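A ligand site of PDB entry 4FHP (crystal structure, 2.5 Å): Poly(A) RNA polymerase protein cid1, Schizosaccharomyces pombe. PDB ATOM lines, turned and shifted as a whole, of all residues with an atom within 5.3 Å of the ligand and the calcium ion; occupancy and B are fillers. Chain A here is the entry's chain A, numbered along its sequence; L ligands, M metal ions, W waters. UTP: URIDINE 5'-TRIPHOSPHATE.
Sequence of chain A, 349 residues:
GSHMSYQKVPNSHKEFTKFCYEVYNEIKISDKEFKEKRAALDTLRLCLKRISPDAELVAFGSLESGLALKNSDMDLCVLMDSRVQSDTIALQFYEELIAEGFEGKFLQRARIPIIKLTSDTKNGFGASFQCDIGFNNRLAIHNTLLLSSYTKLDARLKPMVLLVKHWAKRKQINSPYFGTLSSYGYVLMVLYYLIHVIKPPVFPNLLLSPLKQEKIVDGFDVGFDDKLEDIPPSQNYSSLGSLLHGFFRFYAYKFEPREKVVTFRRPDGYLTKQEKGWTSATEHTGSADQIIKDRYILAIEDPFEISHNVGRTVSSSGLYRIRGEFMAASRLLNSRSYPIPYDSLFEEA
The backbone carbonyl oxygen of Ala 140 sits at hydrogen-bond distance from an oxygen (O2') of the ligand, at 3.2 Å. NZ of Lys 169 is in salt-bridge range of O1G of the ligand (3.0 Å). The side-chain amino group (NZ) of Lys 165 is in salt-bridge range of an oxygen (O2G) of the ligand, 2.6 Å away. The side-chain hydroxyl (OG) of Ser 183 sits at hydrogen-bond distance from an oxygen (O1G) of the ligand (2.7 Å). An oxygen (O2') of the ligand lies within hydrogen-bond range of the side-chain hydroxyl (OG1) of Thr 144 (3.1 Å). OD1 of Asn 143 lies within hydrogen-bond range of O2' of the ligand. OG of Ser 62 is in hydrogen-bond range of O2G of the ligand, 3.4 Å away. N of Tyr 184 lies within hydrogen-bond range of O1A of the ligand (3.0 Å). The backbone NH (N) of Ser 62 lies close to an oxygen (O1B) of the ligand, at 3.1 Å. A ring nitrogen (NE2) of His 308 sits at hydrogen-bond distance from an oxygen (O4) of the ligand.
The backbone carbonyl oxygen (O) of Ala 140 lies close to the side-chain amide oxygen (OD1) of Asn 143 (3.1 Å). The side-chain amino group of Lys 165 sits at hydrogen-bond distance from the backbone carbonyl oxygen of Leu 67, at 2.7 Å. N of Leu 67 sits at hydrogen-bond distance from O of Ser 62 (2.8 Å). OG1 of Thr 144 lies within hydrogen-bond range of O of Ala 140 (2.9 Å). The side-chain hydroxyl of Thr 144 lies within hydrogen-bond range of the backbone NH of Gly 61, at 3.0 Å. The side-chain hydroxyl (OH) of Tyr 184 lies within hydrogen-bond range of the side-chain amide nitrogen (ND2) of Asn 143. O of Asp 75 is in hydrogen-bond range of N of Phe 60 (2.9 Å). The side-chain hydroxyl of Tyr 184 sits at hydrogen-bond distance from the side-chain carboxylate of Asp 302 (2.7 Å).
Residues that only touch the ligand: Phe 60, Gly 61, Ser 182 and Val 310. Hydrophobic or aromatic side chains that line the ligand: Phe 60, Ala 140, Tyr 184, His 308 and Val 310. Of the 24 residues printed, 15 come within 4 Å of the ligand.
Within 4 Å of the calcium ion: Asp 73 and Asp 75. The nearest printed residue that does not touch the calcium ion is Ser 62 (4.1 Å).
The calcium ion is bound by an oxygen (O3G) of the ligand (2.3 Å), an oxygen (O1B) of the ligand (2.4 Å), water W6 (2.4 Å), the side-chain carboxylate of Asp 75 (2.4 Å), the side-chain carboxylate of Asp 73 (2.5 Å), an oxygen (O2A) of the ligand (2.5 Å) and water W1 (2.6 Å). The calcium ion has seven donor atoms within binding distance.
Water W1 lies within hydrogen-bond range of the side-chain carboxylate of Asp 75 and the side-chain carboxylate of Asp 73. Water W2 lies within hydrogen-bond range of an oxygen (O4) of the ligand, the side-chain hydroxyl of Ser 182 and the backbone carbonyl oxygen of Val 310. Water W5 lies within hydrogen-bond range of the side-chain carboxylate (OD1) of Asp 302 (2.7 Å) and a nitrogen (N3) of the ligand (2.9 Å). Water W7 lies within hydrogen-bond range of O3' of the ligand (3.2 Å) and N of Ser 62 (3.4 Å). Water W4 bridges N of Ser 183 (2.9 Å) and O1A of the ligand (3.3 Å).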
ATOM      1  N   PHE A  60      29.852  12.259  25.689  1.00  0.00           N
ATOM      2  CA  PHE A  60      28.470  11.804  25.748  1.00  0.00           C
ATOM      3  C   PHE A  60      27.844  12.056  24.380  1.00  0.00           C
ATOM      4  O   PHE A  60      28.579  12.357  23.413  1.00  0.00           O
ATOM      5  CB  PHE A  60      27.676  12.433  26.916  1.00  0.00           C
ATOM      6  CG  PHE A  60      27.537  13.942  26.843  1.00  0.00           C
ATOM      7  CD1 PHE A  60      28.527  14.778  27.356  1.00  0.00           C
ATOM      8  CD2 PHE A  60      26.410  14.516  26.278  1.00  0.00           C
ATOM      9  CE1 PHE A  60      28.406  16.149  27.305  1.00  0.00           C
ATOM     10  CE2 PHE A  60      26.263  15.907  26.234  1.00  0.00           C
ATOM     11  CZ  PHE A  60      27.271  16.717  26.743  1.00  0.00           C
ATOM     12  N   GLY A  61      26.530  11.904  24.270  1.00  0.00           N
ATOM     13  CA  GLY A  61      25.842  12.035  22.989  1.00  0.00           C
ATOM     14  C   GLY A  61      26.279  10.962  22.003  1.00  0.00           C
ATOM     15  O   GLY A  61      26.840   9.941  22.402  1.00  0.00           O
ATOM     16  N   SER A  62      26.047  11.238  20.712  1.00  0.00           N
ATOM     17  CA  SER A  62      26.093  10.213  19.666  1.00  0.00           C
ATOM     18  C   SER A  62      27.378   9.402  19.584  1.00  0.00           C
ATOM     19  O   SER A  62      27.326   8.192  19.358  1.00  0.00           O
ATOM     20  CB  SER A  62      25.746  10.813  18.315  1.00  0.00           C
ATOM     21  OG  SER A  62      26.546  11.944  18.076  1.00  0.00           O
ATOM     22  N   LEU A  67      25.727   6.231  18.079  1.00  0.00           N
ATOM     23  CA  LEU A  67      24.627   6.709  17.236  1.00  0.00           C
ATOM     24  C   LEU A  67      25.052   7.880  16.358  1.00  0.00           C
ATOM     25  O   LEU A  67      24.274   8.791  16.070  1.00  0.00           O
ATOM     26  CB  LEU A  67      23.411   7.116  18.087  1.00  0.00           C
ATOM     27  CG  LEU A  67      22.658   6.036  18.874  1.00  0.00           C
ATOM     28  CD1 LEU A  67      21.614   6.668  19.803  1.00  0.00           C
ATOM     29  CD2 LEU A  67      22.025   5.002  17.965  1.00  0.00           C
ATOM     30  N   ALA A  68      26.306   7.827  15.928  1.00  0.00           N
ATOM     31  CA  ALA A  68      26.941   8.905  15.206  1.00  0.00           C
ATOM     32  C   ALA A  68      26.825   8.765  13.700  1.00  0.00           C
ATOM     33  O   ALA A  68      27.117   7.711  13.124  1.00  0.00           O
ATOM     34  CB  ALA A  68      28.395   8.962  15.596  1.00  0.00           C
ATOM     35  N   LEU A  69      26.408   9.847  13.065  1.00  0.00           N
ATOM     36  CA  LEU A  69      26.507   9.989  11.625  1.00  0.00           C
ATOM     37  C   LEU A  69      27.897  10.482  11.257  1.00  0.00           C
ATOM     38  O   LEU A  69      28.648  10.942  12.108  1.00  0.00           O
ATOM     39  CB  LEU A  69      25.466  11.005  11.130  1.00  0.00           C
ATOM     40  CG  LEU A  69      23.984  10.715  11.400  1.00  0.00           C
ATOM     41  CD1 LEU A  69      23.138  11.910  10.995  1.00  0.00           C
ATOM     42  CD2 LEU A  69      23.533   9.495  10.627  1.00  0.00           C
ATOM     43  N   SER A  72      30.468  14.171  12.350  1.00  0.00           N
ATOM     44  CA  SER A  72      29.730  14.300  13.590  1.00  0.00           C
ATOM     45  C   SER A  72      30.370  15.319  14.524  1.00  0.00           C
ATOM     46  O   SER A  72      31.583  15.439  14.570  1.00  0.00           O
ATOM     47  CB  SER A  72      29.684  12.948  14.286  1.00  0.00           C
ATOM     48  OG  SER A  72      28.743  12.984  15.334  1.00  0.00           O
ATOM     49  N   ASP A  73      29.527  16.043  15.265  1.00  0.00           N
ATOM     50  CA  ASP A  73      30.023  16.888  16.344  1.00  0.00           C
ATOM     51  C   ASP A  73      30.300  16.077  17.602  1.00  0.00           C
ATOM     52  O   ASP A  73      29.830  14.942  17.745  1.00  0.00           O
ATOM     53  CB  ASP A  73      29.090  18.094  16.611  1.00  0.00           C
ATOM     54  CG  ASP A  73      27.763  17.726  17.280  1.00  0.00           C
ATOM     55  OD1 ASP A  73      26.870  18.593  17.314  1.00  0.00           O
ATOM     56  OD2 ASP A  73      27.593  16.593  17.781  1.00  0.00           O
ATOM     57  N   ASP A  75      30.216  15.937  21.798  1.00  0.00           N
ATOM     58  CA  ASP A  75      29.692  16.476  23.040  1.00  0.00           C
ATOM     59  C   ASP A  75      30.541  15.928  24.164  1.00  0.00           C
ATOM     60  O   ASP A  75      30.690  14.713  24.331  1.00  0.00           O
ATOM     61  CB  ASP A  75      28.232  16.071  23.239  1.00  0.00           C
ATOM     62  CG  ASP A  75      27.352  16.553  22.108  1.00  0.00           C
ATOM     63  OD1 ASP A  75      27.059  17.769  22.051  1.00  0.00           O
ATOM     64  OD2 ASP A  75      26.949  15.711  21.271  1.00  0.00           O
ATOM     65  N   ALA A 140      23.331  14.428  31.339  1.00  0.00           N
ATOM     66  CA  ALA A 140      23.592  14.072  29.948  1.00  0.00           C
ATOM     67  C   ALA A 140      24.422  12.790  29.823  1.00  0.00           C
ATOM     68  O   ALA A 140      24.216  12.014  28.870  1.00  0.00           O
ATOM     69  CB  ALA A 140      24.272  15.204  29.246  1.00  0.00           C
ATOM     70  N   ILE A 141      25.365  12.585  30.752  1.00  0.00           N
ATOM     71  CA  ILE A 141      26.140  11.342  30.810  1.00  0.00           C
ATOM     72  C   ILE A 141      25.188  10.185  31.073  1.00  0.00           C
ATOM     73  O   ILE A 141      25.248   9.165  30.383  1.00  0.00           O
ATOM     74  CB  ILE A 141      27.235  11.386  31.928  1.00  0.00           C
ATOM     75  CG1 ILE A 141      28.389  12.306  31.520  1.00  0.00           C
ATOM     76  CG2 ILE A 141      27.795   9.966  32.255  1.00  0.00           C
ATOM     77  CD1 ILE A 141      29.133  12.871  32.727  1.00  0.00           C
ATOM     78  N   ASN A 143      21.782   9.922  30.700  1.00  0.00           N
ATOM     79  CA  ASN A 143      20.833   9.668  29.634  1.00  0.00           C
ATOM     80  C   ASN A 143      21.528   9.132  28.373  1.00  0.00           C
ATOM     81  O   ASN A 143      20.910   8.417  27.592  1.00  0.00           O
ATOM     82  CB  ASN A 143      19.903  10.859  29.388  1.00  0.00           C
ATOM     83  CG  ASN A 143      20.553  11.970  28.590  1.00  0.00           C
ATOM     84  OD1 ASN A 143      21.361  11.732  27.696  1.00  0.00           O
ATOM     85  ND2 ASN A 143      20.178  13.209  28.904  1.00  0.00           N
ATOM     86  N   THR A 144      22.818   9.426  28.228  1.00  0.00           N
ATOM     87  CA  THR A 144      23.627   8.728  27.218  1.00  0.00           C
ATOM     88  C   THR A 144      23.856   7.239  27.560  1.00  0.00           C
ATOM     89  O   THR A 144      23.892   6.384  26.661  1.00  0.00           O
ATOM     90  CB  THR A 144      24.975   9.443  26.941  1.00  0.00           C
ATOM     91  OG1 THR A 144      24.725  10.727  26.361  1.00  0.00           O
ATOM     92  CG2 THR A 144      25.820   8.635  25.952  1.00  0.00           C
ATOM     93  N   LEU A 147      20.573   5.433  26.459  1.00  0.00           N
ATOM     94  CA  LEU A 147      20.536   5.224  24.999  1.00  0.00           C
ATOM     95  C   LEU A 147      21.601   4.208  24.584  1.00  0.00           C
ATOM     96  O   LEU A 147      21.361   3.361  23.721  1.00  0.00           O
ATOM     97  CB  LEU A 147      20.769   6.525  24.216  1.00  0.00           C
ATOM     98  CG  LEU A 147      20.041   7.843  24.530  1.00  0.00           C
ATOM     99  CD1 LEU A 147      20.278   8.852  23.397  1.00  0.00           C
ATOM    100  CD2 LEU A 147      18.540   7.691  24.778  1.00  0.00           C
ATOM    101  N   LYS A 165      17.563  10.401  12.023  1.00  0.00           N
ATOM    102  CA  LYS A 165      18.384  11.627  12.164  1.00  0.00           C
ATOM    103  C   LYS A 165      18.684  12.212  10.792  1.00  0.00           C
ATOM    104  O   LYS A 165      18.560  13.414  10.595  1.00  0.00           O
ATOM    105  CB  LYS A 165      19.718  11.356  12.852  1.00  0.00           C
ATOM    106  CG  LYS A 165      19.692  11.188  14.377  1.00  0.00           C
ATOM    107  CD  LYS A 165      21.151  10.893  14.817  1.00  0.00           C
ATOM    108  CE  LYS A 165      21.386  11.257  16.249  1.00  0.00           C
ATOM    109  NZ  LYS A 165      22.761  10.923  16.699  1.00  0.00           N
ATOM    110  N   LYS A 169      17.317  15.851   9.280  1.00  0.00           N
ATOM    111  CA  LYS A 169      18.320  16.797   8.785  1.00  0.00           C
ATOM    112  C   LYS A 169      18.055  17.208   7.348  1.00  0.00           C
ATOM    113  O   LYS A 169      18.099  18.386   7.025  1.00  0.00           O
ATOM    114  CB  LYS A 169      19.723  16.203   8.873  1.00  0.00           C
ATOM    115  CG  LYS A 169      20.454  16.550  10.142  1.00  0.00           C
ATOM    116  CD  LYS A 169      21.774  15.788  10.304  1.00  0.00           C
ATOM    117  CE  LYS A 169      21.690  14.867  11.509  1.00  0.00           C
ATOM    118  NZ  LYS A 169      21.874  15.580  12.822  1.00  0.00           N
ATOM    119  N   ASN A 174      15.427  19.541  11.842  1.00  0.00           N
ATOM    120  CA  ASN A 174      16.418  19.231  12.874  1.00  0.00           C
ATOM    121  C   ASN A 174      17.165  20.484  13.383  1.00  0.00           C
ATOM    122  O   ASN A 174      18.374  20.461  13.560  1.00  0.00           O
ATOM    123  CB  ASN A 174      17.380  18.160  12.307  1.00  0.00           C
ATOM    124  CG  ASN A 174      18.401  17.658  13.314  1.00  0.00           C
ATOM    125  OD1 ASN A 174      19.521  17.347  12.918  1.00  0.00           O
ATOM    126  ND2 ASN A 174      18.028  17.570  14.596  1.00  0.00           N
ATOM    127  N   SER A 182      15.833  19.071  18.311  1.00  0.00           N
ATOM    128  CA  SER A 182      17.157  18.468  18.410  1.00  0.00           C
ATOM    129  C   SER A 182      17.151  16.976  18.059  1.00  0.00           C
ATOM    130  O   SER A 182      16.114  16.304  18.174  1.00  0.00           O
ATOM    131  CB  SER A 182      17.693  18.638  19.820  1.00  0.00           C
ATOM    132  OG  SER A 182      16.831  18.002  20.750  1.00  0.00           O
ATOM    133  N   SER A 183      18.314  16.461  17.651  1.00  0.00           N
ATOM    134  CA  SER A 183      18.478  15.040  17.344  1.00  0.00           C
ATOM    135  C   SER A 183      18.139  14.188  18.553  1.00  0.00           C
ATOM    136  O   SER A 183      17.480  13.148  18.420  1.00  0.00           O
ATOM    137  CB  SER A 183      19.905  14.744  16.900  1.00  0.00           C
ATOM    138  OG  SER A 183      20.319  15.636  15.881  1.00  0.00           O
ATOM    139  N   TYR A 184      18.572  14.639  19.735  1.00  0.00           N
ATOM    140  CA  TYR A 184      18.276  13.932  20.967  1.00  0.00           C
ATOM    141  C   TYR A 184      16.761  13.720  21.120  1.00  0.00           C
ATOM    142  O   TYR A 184      16.323  12.650  21.533  1.00  0.00           O
ATOM    143  CB  TYR A 184      18.864  14.671  22.166  1.00  0.00           C
ATOM    144  CG  TYR A 184      18.500  14.050  23.493  1.00  0.00           C
ATOM    145  CD1 TYR A 184      18.918  12.751  23.818  1.00  0.00           C
ATOM    146  CD2 TYR A 184      17.721  14.742  24.428  1.00  0.00           C
ATOM    147  CE1 TYR A 184      18.575  12.172  25.034  1.00  0.00           C
ATOM    148  CE2 TYR A 184      17.385  14.169  25.642  1.00  0.00           C
ATOM    149  CZ  TYR A 184      17.804  12.877  25.943  1.00  0.00           C
ATOM    150  OH  TYR A 184      17.460  12.308  27.145  1.00  0.00           O
ATOM    151  N   VAL A 187      15.591  10.944  18.972  1.00  0.00           N
ATOM    152  CA  VAL A 187      15.979   9.669  19.556  1.00  0.00           C
ATOM    153  C   VAL A 187      14.926   9.223  20.560  1.00  0.00           C
ATOM    154  O   VAL A 187      14.479   8.070  20.547  1.00  0.00           O
ATOM    155  CB  VAL A 187      17.347   9.709  20.224  1.00  0.00           C
ATOM    156  CG1 VAL A 187      17.639   8.367  20.914  1.00  0.00           C
ATOM    157  CG2 VAL A 187      18.437  10.019  19.186  1.00  0.00           C
ATOM    158  N   ASP A 302      11.924  14.635  29.282  1.00  0.00           N
ATOM    159  CA  ASP A 302      13.178  13.876  29.408  1.00  0.00           C
ATOM    160  C   ASP A 302      12.923  12.671  30.332  1.00  0.00           C
ATOM    161  O   ASP A 302      12.144  12.776  31.287  1.00  0.00           O
ATOM    162  CB  ASP A 302      14.277  14.750  29.982  1.00  0.00           C
ATOM    163  CG  ASP A 302      15.639  14.073  29.922  1.00  0.00           C
ATOM    164  OD1 ASP A 302      16.241  14.048  28.810  1.00  0.00           O
ATOM    165  OD2 ASP A 302      16.112  13.582  30.972  1.00  0.00           O
ATOM    166  N   HIS A 308      12.272  19.042  32.329  1.00  0.00           N
ATOM    167  CA  HIS A 308      12.798  19.562  31.070  1.00  0.00           C
ATOM    168  C   HIS A 308      12.031  19.030  29.865  1.00  0.00           C
ATOM    169  O   HIS A 308      12.033  17.833  29.566  1.00  0.00           O
ATOM    170  CB  HIS A 308      14.290  19.228  30.959  1.00  0.00           C
ATOM    171  CG  HIS A 308      14.891  19.544  29.632  1.00  0.00           C
ATOM    172  ND1 HIS A 308      14.846  20.802  29.071  1.00  0.00           N
ATOM    173  CD2 HIS A 308      15.592  18.778  28.762  1.00  0.00           C
ATOM    174  CE1 HIS A 308      15.461  20.787  27.903  1.00  0.00           C
ATOM    175  NE2 HIS A 308      15.938  19.566  27.699  1.00  0.00           N
ATOM    176  N   VAL A 310      12.184  18.436  26.365  1.00  0.00           N
ATOM    177  CA  VAL A 310      13.148  18.320  25.288  1.00  0.00           C
ATOM    178  C   VAL A 310      12.690  19.028  23.997  1.00  0.00           C
ATOM    179  O   VAL A 310      13.514  19.573  23.249  1.00  0.00           O
ATOM    180  CB  VAL A 310      13.498  16.828  25.038  1.00  0.00           C
ATOM    181  CG1 VAL A 310      14.512  16.675  23.915  1.00  0.00           C
ATOM    182  CG2 VAL A 310      14.030  16.190  26.319  1.00  0.00           C
HETATM  183  PA  UTP L   1      22.306  15.882  20.348  1.00  0.00           P
HETATM  184  O1A UTP L   1      20.972  16.480  20.093  1.00  0.00           O
HETATM  185  O2A UTP L   1      23.358  16.500  19.520  1.00  0.00           O
HETATM  186  O3A UTP L   1      22.240  14.299  20.149  1.00  0.00           O
HETATM  187  O5' UTP L   1      22.613  16.035  21.914  1.00  0.00           O
HETATM  188  PB  UTP L   1      23.193  13.525  19.097  1.00  0.00           P
HETATM  189  O1B UTP L   1      24.615  13.721  19.466  1.00  0.00           O
HETATM  190  O2B UTP L   1      22.877  12.083  19.185  1.00  0.00           O
HETATM  191  O3B UTP L   1      22.813  14.048  17.752  1.00  0.00           O
HETATM  192  PG  UTP L   1      23.790  14.361  16.503  1.00  0.00           P
HETATM  193  O1G UTP L   1      22.981  15.220  15.559  1.00  0.00           O
HETATM  194  O2G UTP L   1      24.105  12.983  15.976  1.00  0.00           O
HETATM  195  O3G UTP L   1      24.956  15.077  17.121  1.00  0.00           O
HETATM  196  C5' UTP L   1      23.760  15.405  22.453  1.00  0.00           C
HETATM  197  C4' UTP L   1      23.519  14.919  23.871  1.00  0.00           C
HETATM  198  O4' UTP L   1      23.255  15.991  24.756  1.00  0.00           O
HETATM  199  C1' UTP L   1      22.330  15.595  25.752  1.00  0.00           C
HETATM  200  C2' UTP L   1      22.061  14.112  25.511  1.00  0.00           C
HETATM  201  O2' UTP L   1      22.990  13.327  26.249  1.00  0.00           O
HETATM  202  C3' UTP L   1      22.334  13.981  24.035  1.00  0.00           C
HETATM  203  O3' UTP L   1      22.645  12.647  23.706  1.00  0.00           O
HETATM  204  N1  UTP L   1      21.062  16.356  25.627  1.00  0.00           N
HETATM  205  C6  UTP L   1      20.811  17.177  24.542  1.00  0.00           C
HETATM  206  C2  UTP L   1      20.210  16.439  26.735  1.00  0.00           C
HETATM  207  O2  UTP L   1      20.482  15.878  27.797  1.00  0.00           O
HETATM  208  N3  UTP L   1      19.031  17.150  26.649  1.00  0.00           N
HETATM  209  C4  UTP L   1      18.678  17.791  25.485  1.00  0.00           C
HETATM  210  O4  UTP L   1      17.619  18.417  25.456  1.00  0.00           O
HETATM  211  C5  UTP L   1      19.527  17.732  24.380  1.00  0.00           C
HETATM  212 CA    CA M   1      25.745  15.763  19.172  1.00  0.00          CA
HETATM  213  O   HOH W   1      25.347  18.302  19.796  1.00  0.00           O
HETATM  214  O   HOH W   2      16.929  19.266  23.182  1.00  0.00           O
HETATM  215  O   HOH W   3      26.579  15.713  14.919  1.00  0.00           O
HETATM  216  O   HOH W   4      20.402  18.518  17.559  1.00  0.00           O
HETATM  217  O   HOH W   5      17.518  16.419  29.008  1.00  0.00           O
HETATM  218  O   HOH W   6      27.395  14.045  18.817  1.00  0.00           O
HETATM  219  O   HOH W   7      22.999  10.082  21.806  1.00  0.00           O
